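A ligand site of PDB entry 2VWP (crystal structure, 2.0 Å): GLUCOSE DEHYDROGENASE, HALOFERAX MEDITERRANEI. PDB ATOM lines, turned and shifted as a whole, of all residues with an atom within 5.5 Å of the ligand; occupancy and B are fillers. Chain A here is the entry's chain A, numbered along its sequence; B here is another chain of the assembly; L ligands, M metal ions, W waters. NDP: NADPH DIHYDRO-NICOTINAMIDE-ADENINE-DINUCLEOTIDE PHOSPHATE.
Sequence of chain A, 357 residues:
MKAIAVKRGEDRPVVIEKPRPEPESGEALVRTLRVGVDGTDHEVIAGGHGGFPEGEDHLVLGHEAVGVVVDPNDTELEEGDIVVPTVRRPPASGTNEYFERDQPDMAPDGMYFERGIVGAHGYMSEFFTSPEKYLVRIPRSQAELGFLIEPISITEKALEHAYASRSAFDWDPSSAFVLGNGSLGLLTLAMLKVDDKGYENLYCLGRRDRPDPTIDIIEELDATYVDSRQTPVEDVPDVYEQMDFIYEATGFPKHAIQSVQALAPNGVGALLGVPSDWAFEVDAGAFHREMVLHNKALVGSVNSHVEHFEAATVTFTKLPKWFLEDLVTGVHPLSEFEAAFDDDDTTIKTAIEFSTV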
ATOM      1  N   ASP A  38      -3.398  11.934  14.010  1.00  0.00           N
ATOM      2  CA  ASP A  38      -4.541  12.224  14.831  1.00  0.00           C
ATOM      3  C   ASP A  38      -4.492  11.366  16.098  1.00  0.00           C
ATOM      4  O   ASP A  38      -3.746  10.382  16.147  1.00  0.00           O
ATOM      5  CB  ASP A  38      -5.789  11.856  14.032  1.00  0.00           C
ATOM      6  CG  ASP A  38      -7.029  12.207  14.738  1.00  0.00           C
ATOM      7  OD1 ASP A  38      -7.260  13.409  14.932  1.00  0.00           O
ATOM      8  OD2 ASP A  38      -7.775  11.289  15.124  1.00  0.00           O
ATOM      9  N   GLY A  39      -5.291  11.731  17.107  1.00  0.00           N
ATOM     10  CA  GLY A  39      -5.544  10.914  18.299  1.00  0.00           C
ATOM     11  C   GLY A  39      -5.886   9.462  18.022  1.00  0.00           C
ATOM     12  O   GLY A  39      -5.412   8.578  18.729  1.00  0.00           O
ATOM     13  N   GLU A  43      -4.323   6.044  19.517  1.00  0.00           N
ATOM     14  CA  GLU A  43      -5.145   4.960  20.080  1.00  0.00           C
ATOM     15  C   GLU A  43      -4.835   3.579  19.464  1.00  0.00           C
ATOM     16  O   GLU A  43      -4.834   2.565  20.187  1.00  0.00           O
ATOM     17  CB  GLU A  43      -6.638   5.250  19.915  1.00  0.00           C
ATOM     18  CG  GLU A  43      -7.177   6.474  20.644  1.00  0.00           C
ATOM     19  CD  GLU A  43      -8.481   6.972  20.029  1.00  0.00           C
ATOM     20  OE1 GLU A  43      -9.278   6.111  19.557  1.00  0.00           O
ATOM     21  OE2 GLU A  43      -8.717   8.205  20.014  1.00  0.00           O
ATOM     22  N   ILE A 154     -14.989  17.150   9.498  1.00  0.00           N
ATOM     23  CA  ILE A 154     -15.648  16.629  10.683  1.00  0.00           C
ATOM     24  C   ILE A 154     -16.539  17.714  11.334  1.00  0.00           C
ATOM     25  O   ILE A 154     -17.712  17.468  11.695  1.00  0.00           O
ATOM     26  CB  ILE A 154     -14.614  16.118  11.730  1.00  0.00           C
ATOM     27  CG1 ILE A 154     -13.829  14.906  11.192  1.00  0.00           C
ATOM     28  CG2 ILE A 154     -15.290  15.845  13.078  1.00  0.00           C
ATOM     29  CD1 ILE A 154     -14.666  13.596  11.005  1.00  0.00           C
ATOM     30  N   LEU A 179     -15.247  23.309  23.589  1.00  0.00           N
ATOM     31  CA  LEU A 179     -14.673  22.599  24.686  1.00  0.00           C
ATOM     32  C   LEU A 179     -13.545  21.748  24.131  1.00  0.00           C
ATOM     33  O   LEU A 179     -13.806  20.820  23.352  1.00  0.00           O
ATOM     34  CB  LEU A 179     -15.722  21.734  25.394  1.00  0.00           C
ATOM     35  CG  LEU A 179     -17.109  22.330  25.639  1.00  0.00           C
ATOM     36  CD1 LEU A 179     -17.986  21.346  26.416  1.00  0.00           C
ATOM     37  CD2 LEU A 179     -17.010  23.638  26.374  1.00  0.00           C
ATOM     38  N   GLY A 180     -12.302  22.057  24.492  1.00  0.00           N
ATOM     39  CA  GLY A 180     -11.175  21.284  23.958  1.00  0.00           C
ATOM     40  C   GLY A 180     -10.214  22.120  23.141  1.00  0.00           C
ATOM     41  O   GLY A 180     -10.636  22.919  22.294  1.00  0.00           O
ATOM     42  N   ASN A 181      -8.921  21.908  23.396  1.00  0.00           N
ATOM     43  CA  ASN A 181      -7.842  22.657  22.732  1.00  0.00           C
ATOM     44  C   ASN A 181      -6.897  21.714  21.967  1.00  0.00           C
ATOM     45  O   ASN A 181      -5.723  22.017  21.786  1.00  0.00           O
ATOM     46  CB  ASN A 181      -7.064  23.490  23.758  1.00  0.00           C
ATOM     47  CG  ASN A 181      -6.461  22.626  24.884  1.00  0.00           C
ATOM     48  OD1 ASN A 181      -7.061  21.654  25.339  1.00  0.00           O
ATOM     49  ND2 ASN A 181      -5.245  22.973  25.313  1.00  0.00           N
ATOM     50  N   GLY A 182      -7.423  20.565  21.544  1.00  0.00           N
ATOM     51  CA  GLY A 182      -6.714  19.698  20.611  1.00  0.00           C
ATOM     52  C   GLY A 182      -6.852  20.320  19.216  1.00  0.00           C
ATOM     53  O   GLY A 182      -7.479  21.367  19.080  1.00  0.00           O
ATOM     54  N   SER A 183      -6.265  19.716  18.203  1.00  0.00           N
ATOM     55  CA  SER A 183      -6.307  20.317  16.850  1.00  0.00           C
ATOM     56  C   SER A 183      -7.738  20.468  16.330  1.00  0.00           C
ATOM     57  O   SER A 183      -8.053  21.458  15.666  1.00  0.00           O
ATOM     58  CB  SER A 183      -5.411  19.539  15.866  1.00  0.00           C
ATOM     59  OG  SER A 183      -5.817  18.195  15.809  1.00  0.00           O
ATOM     60  N   LEU A 184      -8.620  19.512  16.661  1.00  0.00           N
ATOM     61  CA  LEU A 184     -10.035  19.651  16.277  1.00  0.00           C
ATOM     62  C   LEU A 184     -10.710  20.861  16.917  1.00  0.00           C
ATOM     63  O   LEU A 184     -11.407  21.633  16.239  1.00  0.00           O
ATOM     64  CB  LEU A 184     -10.857  18.391  16.554  1.00  0.00           C
ATOM     65  CG  LEU A 184     -12.283  18.385  15.968  1.00  0.00           C
ATOM     66  CD1 LEU A 184     -12.238  18.369  14.425  1.00  0.00           C
ATOM     67  CD2 LEU A 184     -13.107  17.205  16.503  1.00  0.00           C
ATOM     68  N   GLY A 185     -10.532  21.013  18.238  1.00  0.00           N
ATOM     69  CA  GLY A 185     -11.105  22.145  18.929  1.00  0.00           C
ATOM     70  C   GLY A 185     -10.596  23.456  18.337  1.00  0.00           C
ATOM     71  O   GLY A 185     -11.373  24.407  18.160  1.00  0.00           O
ATOM     72  N   LEU A 205     -12.271  26.051  25.899  1.00  0.00           N
ATOM     73  CA  LEU A 205     -11.928  25.431  27.167  1.00  0.00           C
ATOM     74  C   LEU A 205     -10.701  24.547  27.063  1.00  0.00           C
ATOM     75  O   LEU A 205     -10.585  23.741  26.136  1.00  0.00           O
ATOM     76  CB  LEU A 205     -13.132  24.594  27.685  1.00  0.00           C
ATOM     77  CG  LEU A 205     -12.992  24.019  29.099  1.00  0.00           C
ATOM     78  CD1 LEU A 205     -13.581  24.999  30.089  1.00  0.00           C
ATOM     79  CD2 LEU A 205     -13.649  22.643  29.224  1.00  0.00           C
ATOM     80  N   GLY A 206      -9.786  24.720  28.000  1.00  0.00           N
ATOM     81  CA  GLY A 206      -8.603  23.885  28.097  1.00  0.00           C
ATOM     82  C   GLY A 206      -8.206  23.799  29.559  1.00  0.00           C
ATOM     83  O   GLY A 206      -8.941  24.265  30.446  1.00  0.00           O
ATOM     84  N   ARG A 207      -7.040  23.231  29.827  1.00  0.00           N
ATOM     85  CA  ARG A 207      -6.521  23.154  31.202  1.00  0.00           C
ATOM     86  C   ARG A 207      -4.978  23.233  31.224  1.00  0.00           C
ATOM     87  O   ARG A 207      -4.309  22.434  31.865  1.00  0.00           O
ATOM     88  CB  ARG A 207      -7.038  21.899  31.897  1.00  0.00           C
ATOM     89  CG  ARG A 207      -6.805  20.633  31.138  1.00  0.00           C
ATOM     90  CD  ARG A 207      -7.526  19.481  31.756  1.00  0.00           C
ATOM     91  NE  ARG A 207      -7.237  18.248  31.017  1.00  0.00           N
ATOM     92  CZ  ARG A 207      -7.767  17.067  31.287  1.00  0.00           C
ATOM     93  NH1 ARG A 207      -8.622  16.955  32.306  1.00  0.00           N
ATOM     94  NH2 ARG A 207      -7.454  15.999  30.565  1.00  0.00           N
ATOM     95  N   ARG A 208      -4.439  24.209  30.497  1.00  0.00           N
ATOM     96  CA  ARG A 208      -2.992  24.363  30.366  1.00  0.00           C
ATOM     97  C   ARG A 208      -2.510  25.514  31.217  1.00  0.00           C
ATOM     98  O   ARG A 208      -3.265  26.450  31.475  1.00  0.00           O
ATOM     99  CB  ARG A 208      -2.606  24.630  28.897  1.00  0.00           C
ATOM    100  CG  ARG A 208      -3.102  23.557  27.936  1.00  0.00           C
ATOM    101  CD  ARG A 208      -2.294  22.294  28.110  1.00  0.00           C
ATOM    102  NE  ARG A 208      -2.688  21.236  27.182  1.00  0.00           N
ATOM    103  CZ  ARG A 208      -2.238  21.099  25.931  1.00  0.00           C
ATOM    104  NH1 ARG A 208      -1.395  21.989  25.393  1.00  0.00           N
ATOM    105  NH2 ARG A 208      -2.668  20.073  25.194  1.00  0.00           N
ATOM    106  N   SER A 228     -10.413  25.204  32.683  1.00  0.00           N
ATOM    107  CA  SER A 228     -11.435  24.450  33.407  1.00  0.00           C
ATOM    108  C   SER A 228     -11.106  24.229  34.890  1.00  0.00           C
ATOM    109  O   SER A 228     -11.999  24.019  35.700  1.00  0.00           O
ATOM    110  CB  SER A 228     -11.699  23.113  32.707  1.00  0.00           C
ATOM    111  OG  SER A 228     -10.582  22.251  32.823  1.00  0.00           O
ATOM    112  N   GLU A 248     -18.467  20.366  21.636  1.00  0.00           N
ATOM    113  CA  GLU A 248     -17.714  19.529  22.551  1.00  0.00           C
ATOM    114  C   GLU A 248     -16.672  18.674  21.828  1.00  0.00           C
ATOM    115  O   GLU A 248     -17.013  17.846  20.968  1.00  0.00           O
ATOM    116  CB  GLU A 248     -18.652  18.685  23.414  1.00  0.00           C
ATOM    117  CG  GLU A 248     -17.942  17.734  24.372  1.00  0.00           C
ATOM    118  CD  GLU A 248     -17.521  16.447  23.730  1.00  0.00           C
ATOM    119  OE1 GLU A 248     -18.322  15.843  22.995  1.00  0.00           O
ATOM    120  OE2 GLU A 248     -16.379  15.996  23.974  1.00  0.00           O
ATOM    121  N   ALA A 249     -15.402  18.876  22.182  1.00  0.00           N
ATOM    122  CA  ALA A 249     -14.278  18.132  21.605  1.00  0.00           C
ATOM    123  C   ALA A 249     -13.235  17.768  22.687  1.00  0.00           C
ATOM    124  O   ALA A 249     -12.017  17.901  22.468  1.00  0.00           O
ATOM    125  CB  ALA A 249     -13.615  18.953  20.476  1.00  0.00           C
ATOM    126  N   THR A 250     -13.730  17.337  23.851  1.00  0.00           N
ATOM    127  CA  THR A 250     -12.843  16.915  24.954  1.00  0.00           C
ATOM    128  C   THR A 250     -12.854  15.406  25.140  1.00  0.00           C
ATOM    129  O   THR A 250     -11.873  14.813  25.563  1.00  0.00           O
ATOM    130  CB  THR A 250     -13.218  17.565  26.317  1.00  0.00           C
ATOM    131  OG1 THR A 250     -14.587  17.281  26.630  1.00  0.00           O
ATOM    132  CG2 THR A 250     -13.002  19.080  26.287  1.00  0.00           C
ATOM    133  N   GLY A 251     -13.991  14.786  24.821  1.00  0.00           N
ATOM    134  CA  GLY A 251     -14.225  13.389  25.174  1.00  0.00           C
ATOM    135  C   GLY A 251     -14.451  13.179  26.676  1.00  0.00           C
ATOM    136  O   GLY A 251     -14.318  12.062  27.161  1.00  0.00           O
ATOM    137  N   PHE A 252     -14.778  14.254  27.383  1.00  0.00           N
ATOM    138  CA  PHE A 252     -15.049  14.235  28.843  1.00  0.00           C
ATOM    139  C   PHE A 252     -16.566  14.124  29.113  1.00  0.00           C
ATOM    140  O   PHE A 252     -17.285  15.094  28.882  1.00  0.00           O
ATOM    141  CB  PHE A 252     -14.491  15.533  29.430  1.00  0.00           C
ATOM    142  CG  PHE A 252     -14.304  15.521  30.940  1.00  0.00           C
ATOM    143  CD1 PHE A 252     -13.474  14.564  31.558  1.00  0.00           C
ATOM    144  CD2 PHE A 252     -14.880  16.513  31.740  1.00  0.00           C
ATOM    145  CE1 PHE A 252     -13.281  14.581  32.943  1.00  0.00           C
ATOM    146  CE2 PHE A 252     -14.686  16.539  33.129  1.00  0.00           C
ATOM    147  CZ  PHE A 252     -13.892  15.569  33.730  1.00  0.00           C
ATOM    148  N   HIS A 255     -18.808  16.904  30.407  1.00  0.00           N
ATOM    149  CA  HIS A 255     -19.081  18.004  29.496  1.00  0.00           C
ATOM    150  C   HIS A 255     -20.367  17.834  28.689  1.00  0.00           C
ATOM    151  O   HIS A 255     -21.029  18.815  28.401  1.00  0.00           O
ATOM    152  CB  HIS A 255     -17.902  18.263  28.567  1.00  0.00           C
ATOM    153  CG  HIS A 255     -16.705  18.837  29.264  1.00  0.00           C
ATOM    154  ND1 HIS A 255     -15.425  18.710  28.774  1.00  0.00           N
ATOM    155  CD2 HIS A 255     -16.594  19.516  30.431  1.00  0.00           C
ATOM    156  CE1 HIS A 255     -14.581  19.310  29.595  1.00  0.00           C
ATOM    157  NE2 HIS A 255     -15.262  19.798  30.610  1.00  0.00           N
ATOM    158  N   LEU A 271     -21.925  17.377  20.114  1.00  0.00           N
ATOM    159  CA  LEU A 271     -21.036  16.445  20.770  1.00  0.00           C
ATOM    160  C   LEU A 271     -20.235  15.670  19.736  1.00  0.00           C
ATOM    161  O   LEU A 271     -20.808  15.091  18.812  1.00  0.00           O
ATOM    162  CB  LEU A 271     -21.835  15.470  21.652  1.00  0.00           C
ATOM    163  CG  LEU A 271     -22.828  16.069  22.657  1.00  0.00           C
ATOM    164  CD1 LEU A 271     -23.499  14.924  23.387  1.00  0.00           C
ATOM    165  CD2 LEU A 271     -22.143  17.030  23.640  1.00  0.00           C
ATOM    166  N   LEU A 272     -18.900  15.698  19.899  1.00  0.00           N
ATOM    167  CA  LEU A 272     -17.953  14.999  19.011  1.00  0.00           C
ATOM    168  C   LEU A 272     -17.094  13.995  19.770  1.00  0.00           C
ATOM    169  O   LEU A 272     -16.493  13.086  19.164  1.00  0.00           O
ATOM    170  CB  LEU A 272     -17.020  16.002  18.293  1.00  0.00           C
ATOM    171  CG  LEU A 272     -17.495  16.920  17.152  1.00  0.00           C
ATOM    172  CD1 LEU A 272     -17.690  16.109  15.865  1.00  0.00           C
ATOM    173  CD2 LEU A 272     -18.743  17.777  17.487  1.00  0.00           C
ATOM    174  N   GLY A 273     -17.032  14.163  21.087  1.00  0.00           N
ATOM    175  CA  GLY A 273     -16.179  13.313  21.945  1.00  0.00           C
ATOM    176  C   GLY A 273     -16.580  11.860  21.998  1.00  0.00           C
ATOM    177  O   GLY A 273     -17.769  11.525  21.913  1.00  0.00           O
ATOM    178  N   VAL A 274     -15.582  10.984  22.131  1.00  0.00           N
ATOM    179  CA  VAL A 274     -15.834   9.550  22.205  1.00  0.00           C
ATOM    180  C   VAL A 274     -15.264   8.947  23.516  1.00  0.00           C
ATOM    181  O   VAL A 274     -14.157   8.411  23.522  1.00  0.00           O
ATOM    182  CB  VAL A 274     -15.301   8.790  20.941  1.00  0.00           C
ATOM    183  CG1 VAL A 274     -15.782   7.343  20.931  1.00  0.00           C
ATOM    184  CG2 VAL A 274     -15.728   9.487  19.651  1.00  0.00           C
ATOM    185  N   SER A 301     -22.341  13.826  16.515  1.00  0.00           N
ATOM    186  CA  SER A 301     -21.913  13.750  15.116  1.00  0.00           C
ATOM    187  C   SER A 301     -20.604  12.966  14.996  1.00  0.00           C
ATOM    188  O   SER A 301     -19.690  13.136  15.809  1.00  0.00           O
ATOM    189  CB  SER A 301     -21.776  15.154  14.514  1.00  0.00           C
ATOM    190  OG  SER A 301     -21.355  15.098  13.171  1.00  0.00           O
ATOM    191  N   VAL A 302     -20.513  12.138  13.966  1.00  0.00           N
ATOM    192  CA  VAL A 302     -19.298  11.361  13.730  1.00  0.00           C
ATOM    193  C   VAL A 302     -19.008  11.294  12.240  1.00  0.00           C
ATOM    194  O   VAL A 302     -19.939  11.231  11.431  1.00  0.00           O
ATOM    195  CB  VAL A 302     -19.351   9.943  14.414  1.00  0.00           C
ATOM    196  CG1 VAL A 302     -20.451   9.070  13.811  1.00  0.00           C
ATOM    197  CG2 VAL A 302     -17.996   9.229  14.331  1.00  0.00           C
ATOM    198  N   ASN A 303     -17.717  11.361  11.883  1.00  0.00           N
ATOM    199  CA  ASN A 303     -17.276  11.180  10.504  1.00  0.00           C
ATOM    200  C   ASN A 303     -17.779  12.371   9.653  1.00  0.00           C
ATOM    201  O   ASN A 303     -18.118  13.438  10.192  1.00  0.00           O
ATOM    202  CB  ASN A 303     -17.753   9.794   9.969  1.00  0.00           C
ATOM    203  CG  ASN A 303     -17.068   9.369   8.665  1.00  0.00           C
ATOM    204  OD1 ASN A 303     -17.731   9.163   7.652  1.00  0.00           O
ATOM    205  ND2 ASN A 303     -15.741   9.200   8.704  1.00  0.00           N
ATOM    206  N   ASP A 345       2.417  18.864  25.059  1.00  0.00           N
ATOM    207  CA  ASP A 345       1.673  20.103  25.047  1.00  0.00           C
ATOM    208  C   ASP A 345       2.021  21.062  23.898  1.00  0.00           C
ATOM    209  O   ASP A 345       1.137  21.748  23.396  1.00  0.00           O
ATOM    210  CB  ASP A 345       1.826  20.829  26.390  1.00  0.00           C
ATOM    211  CG  ASP A 345       0.949  20.238  27.475  1.00  0.00           C
ATOM    212  OD1 ASP A 345       0.324  19.174  27.250  1.00  0.00           O
ATOM    213  OD2 ASP A 345       0.886  20.861  28.557  1.00  0.00           O
ATOM    214  N   VAL B 292     -22.833  10.294  20.070  1.00  0.00           N
ATOM    215  CA  VAL B 292     -21.850  10.679  19.060  1.00  0.00           C
ATOM    216  C   VAL B 292     -21.664   9.622  17.975  1.00  0.00           C
ATOM    217  O   VAL B 292     -21.833   9.910  16.766  1.00  0.00           O
ATOM    218  CB  VAL B 292     -20.483  11.033  19.751  1.00  0.00           C
ATOM    219  CG1 VAL B 292     -19.354  11.214  18.726  1.00  0.00           C
ATOM    220  CG2 VAL B 292     -20.678  12.287  20.617  1.00  0.00           C
HETATM  221  PA  NDP L   1      -7.466  15.728  21.932  1.00  0.00           P
HETATM  222  O1A NDP L   1      -6.126  16.068  21.404  1.00  0.00           O
HETATM  223  O2A NDP L   1      -7.419  14.701  23.028  1.00  0.00           O
HETATM  224  O5B NDP L   1      -8.190  17.062  22.458  1.00  0.00           O
HETATM  225  C5B NDP L   1      -8.925  17.030  23.643  1.00  0.00           C
HETATM  226  C4B NDP L   1      -8.492  18.245  24.445  1.00  0.00           C
HETATM  227  O4B NDP L   1      -9.438  18.404  25.468  1.00  0.00           O
HETATM  228  C3B NDP L   1      -7.110  18.057  25.088  1.00  0.00           C
HETATM  229  O3B NDP L   1      -6.229  19.087  24.653  1.00  0.00           O
HETATM  230  C2B NDP L   1      -7.396  18.080  26.580  1.00  0.00           C
HETATM  231  O2B NDP L   1      -6.508  18.889  27.307  1.00  0.00           O
HETATM  232  C1B NDP L   1      -8.769  18.742  26.658  1.00  0.00           C
HETATM  233  N9A NDP L   1      -9.532  18.288  27.822  1.00  0.00           N
HETATM  234  C8A NDP L   1      -9.896  17.011  28.184  1.00  0.00           C
HETATM  235  N7A NDP L   1     -10.593  17.102  29.353  1.00  0.00           N
HETATM  236  C5A NDP L   1     -10.652  18.412  29.722  1.00  0.00           C
HETATM  237  C6A NDP L   1     -11.213  19.082  30.811  1.00  0.00           C
HETATM  238  N6A NDP L   1     -11.737  18.415  31.840  1.00  0.00           N
HETATM  239  N1A NDP L   1     -11.087  20.465  30.875  1.00  0.00           N
HETATM  240  C2A NDP L   1     -10.427  21.179  29.904  1.00  0.00           C
HETATM  241  N3A NDP L   1      -9.879  20.520  28.845  1.00  0.00           N
HETATM  242  C4A NDP L   1      -9.984  19.168  28.754  1.00  0.00           C
HETATM  243  O3  NDP L   1      -8.379  15.220  20.675  1.00  0.00           O
HETATM  244  PN  NDP L   1      -8.922  16.054  19.374  1.00  0.00           P
HETATM  245  O1N NDP L   1      -9.037  17.517  19.609  1.00  0.00           O
HETATM  246  O2N NDP L   1      -8.196  15.629  18.148  1.00  0.00           O
HETATM  247  O5D NDP L   1     -10.404  15.408  19.391  1.00  0.00           O
HETATM  248  C5D NDP L   1     -11.307  15.761  20.437  1.00  0.00           C
HETATM  249  C4D NDP L   1     -12.313  14.653  20.808  1.00  0.00           C
HETATM  250  O4D NDP L   1     -13.176  14.429  19.699  1.00  0.00           O
HETATM  251  C3D NDP L   1     -11.702  13.301  21.193  1.00  0.00           C
HETATM  252  O3D NDP L   1     -12.473  12.674  22.198  1.00  0.00           O
HETATM  253  C2D NDP L   1     -11.829  12.488  19.930  1.00  0.00           C
HETATM  254  O2D NDP L   1     -12.013  11.113  20.199  1.00  0.00           O
HETATM  255  C1D NDP L   1     -13.089  13.075  19.305  1.00  0.00           C
HETATM  256  N1N NDP L   1     -13.104  13.018  17.841  1.00  0.00           N
HETATM  257  C2N NDP L   1     -14.319  12.758  17.279  1.00  0.00           C
HETATM  258  C3N NDP L   1     -14.547  12.843  15.912  1.00  0.00           C
HETATM  259  C7N NDP L   1     -15.934  12.538  15.393  1.00  0.00           C
HETATM  260  O7N NDP L   1     -16.095  12.367  14.013  1.00  0.00           O
HETATM  261  N7N NDP L   1     -16.981  12.439  16.238  1.00  0.00           N
HETATM  262  C4N NDP L   1     -13.421  13.217  14.968  1.00  0.00           C
HETATM  263  C5N NDP L   1     -12.130  13.491  15.704  1.00  0.00           C
HETATM  264  C6N NDP L   1     -12.019  13.380  17.094  1.00  0.00           C
HETATM  265  P2B NDP L   1      -5.128  18.344  27.925  1.00  0.00           P
HETATM  266  O1X NDP L   1      -4.210  17.871  26.826  1.00  0.00           O
HETATM  267  O2X NDP L   1      -5.404  17.135  28.805  1.00  0.00           O
HETATM  268  O3X NDP L   1      -4.613  19.554  28.680  1.00  0.00           O
HETATM  269 ZN    ZN M   1      -9.354  13.067  11.331  1.00  0.00          ZN
HETATM  270  O   HOH W   1      -3.564  16.233  24.763  1.00  0.00           O
HETATM  271  O   HOH W   2      -5.895  21.521  27.870  1.00  0.00           O
HETATM  272  O   HOH W   3      -7.945  14.596  27.024  1.00  0.00           O
HETATM  273  O   HOH W   4      -8.289  11.799  21.285  1.00  0.00           O
HETATM  274  O   HOH W   5     -11.605   8.490  21.371  1.00  0.00           O
HETATM  275  O   HOH W   6     -10.729  13.936  12.772  1.00  0.00           O
HETATM  276  O   HOH W   7     -11.909   9.925  17.572  1.00  0.00           O
HETATM  277  O   HOH W   8     -10.045  19.291  20.914  1.00  0.00           O
HETATM  278  O   HOH W   9      -8.557  12.482  18.251  1.00  0.00           O
HETATM  279  O   HOH W  10     -13.250  19.786  34.078  1.00  0.00           O
HETATM  280  O   HOH W  11      -9.146  15.107  15.430  1.00  0.00           O
HETATM  281  O   HOH W  12      -4.618  18.023  22.873  1.00  0.00           O
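A nitrogen (N7N) of the ligand is in hydrogen-bond range of the backbone carbonyl oxygen of Ser 301 (2.8 Å).
The guanidinium group of Arg 207 is in salt-bridge range of an oxygen (O2X) of the ligand (2.9 Å).
O3B of the ligand sits at hydrogen-bond distance from OD1 of Asn 181 (2.8 Å).
An oxygen (O7N) of the ligand lies within hydrogen-bond range of the backbone NH (N) of Asn 303, 2.9 Å away.
N1A of the ligand is in hydrogen-bond range of OG of Ser 228, 2.7 Å away.
The backbone carbonyl oxygen (O) of Leu 272 sits close to a nitrogen (N7N) of the ligand (3.0 Å).
NE of Arg 208 is in salt-bridge range of O3X of the ligand (3.0 Å).
O of Leu 205 sits at hydrogen-bond distance from N of Gly 180 (2.9 Å).
The side-chain hydroxyl (OG1) of Thr 250 sits at hydrogen-bond distance from the backbone NH (N) of Phe 252, 3.1 Å away.
The backbone NH (N) of Gly 273 is in hydrogen-bond range of the side-chain carboxylate (OE1) of Glu 248, at 2.9 Å.
The backbone NH of Leu 272 is in hydrogen-bond range of the backbone carbonyl oxygen of Glu 248, at 3.1 Å.
The side-chain carboxylate (OE2) of Glu 248 lies within hydrogen-bond range of the backbone NH (N) of Thr 250.
A ring nitrogen (ND1) of His 255 lies within hydrogen-bond range of the side-chain hydroxyl of Thr 250.
O of Leu 179 lies within hydrogen-bond range of N of Ala 249 (2.8 Å).
The backbone NH of Ser 228 lies within hydrogen-bond range of the backbone carbonyl oxygen of Gly 206.
Ile 154 touches the ligand.
CA of Gly 180 touches O4B of the ligand (3.7 Å).
Gly 182 touches the ligand.
Ser 183 touches the ligand (N to O1N, 3.8 Å).
Leu 184 touches the ligand.
CD2 of Leu 205 touches C2A of the ligand, 3.6 Å away.
Gly 206 touches the ligand.
Ala 249 touches the ligand.
Thr 250 touches the ligand.
Gly 251 touches the ligand.
CD2 of Phe 252 touches N6A of the ligand, at 3.7 Å.
His 255 touches the ligand (CE1 to C6A, 3.6 Å).
Gly 273 touches the ligand.
N of Val 274 touches O3D of the ligand, 3.5 Å away.
Val 302 touches the ligand.
CG1 of Val 292 of chain B touches N7N of the ligand, 3.6 Å away.
23 residues have an atom within 4 Å of the ligand: Ile 154, Gly 180, Asn 181, Gly 182, Ser 183, Leu 184, Leu 205, Gly 206, Arg 207, Arg 208, Ser 228, Ala 249, Thr 250, Gly 251, Phe 252, His 255, Leu 272, Gly 273, Val 274, Ser 301, Val 302, Asn 303 and Val 292 of chain B.
Along chain A the residues within 4 Å of the ligand span positions 154 to 303.
Water W8 lies within hydrogen-bond range of O1N of the ligand (2.4 Å), O of Ala 249 (2.9 Å), N of Gly 182 (3.0 Å) and N of Gly 185 (3.2 Å).
Water W2 lies within hydrogen-bond range of O3X of the ligand (2.5 Å), OD1 of Asn 181 (2.8 Å), N of Arg 207 (2.8 Å) and NE of Arg 208 (3.3 Å).
Water W5 lies within hydrogen-bond range of an oxygen (O2D) of the ligand (2.9 Å), the side-chain carboxylate (OE2) of Glu 43 (3.2 Å) and the backbone carbonyl oxygen (O) of Val 274 (3.3 Å).
Water W11 lies within hydrogen-bond range of OD1 of Asp 38 (2.6 Å) and O2N of the ligand (2.9 Å).
Water W9 bridges O2N of the ligand (3.2 Å) and OD2 of Asp 38 (3.4 Å).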
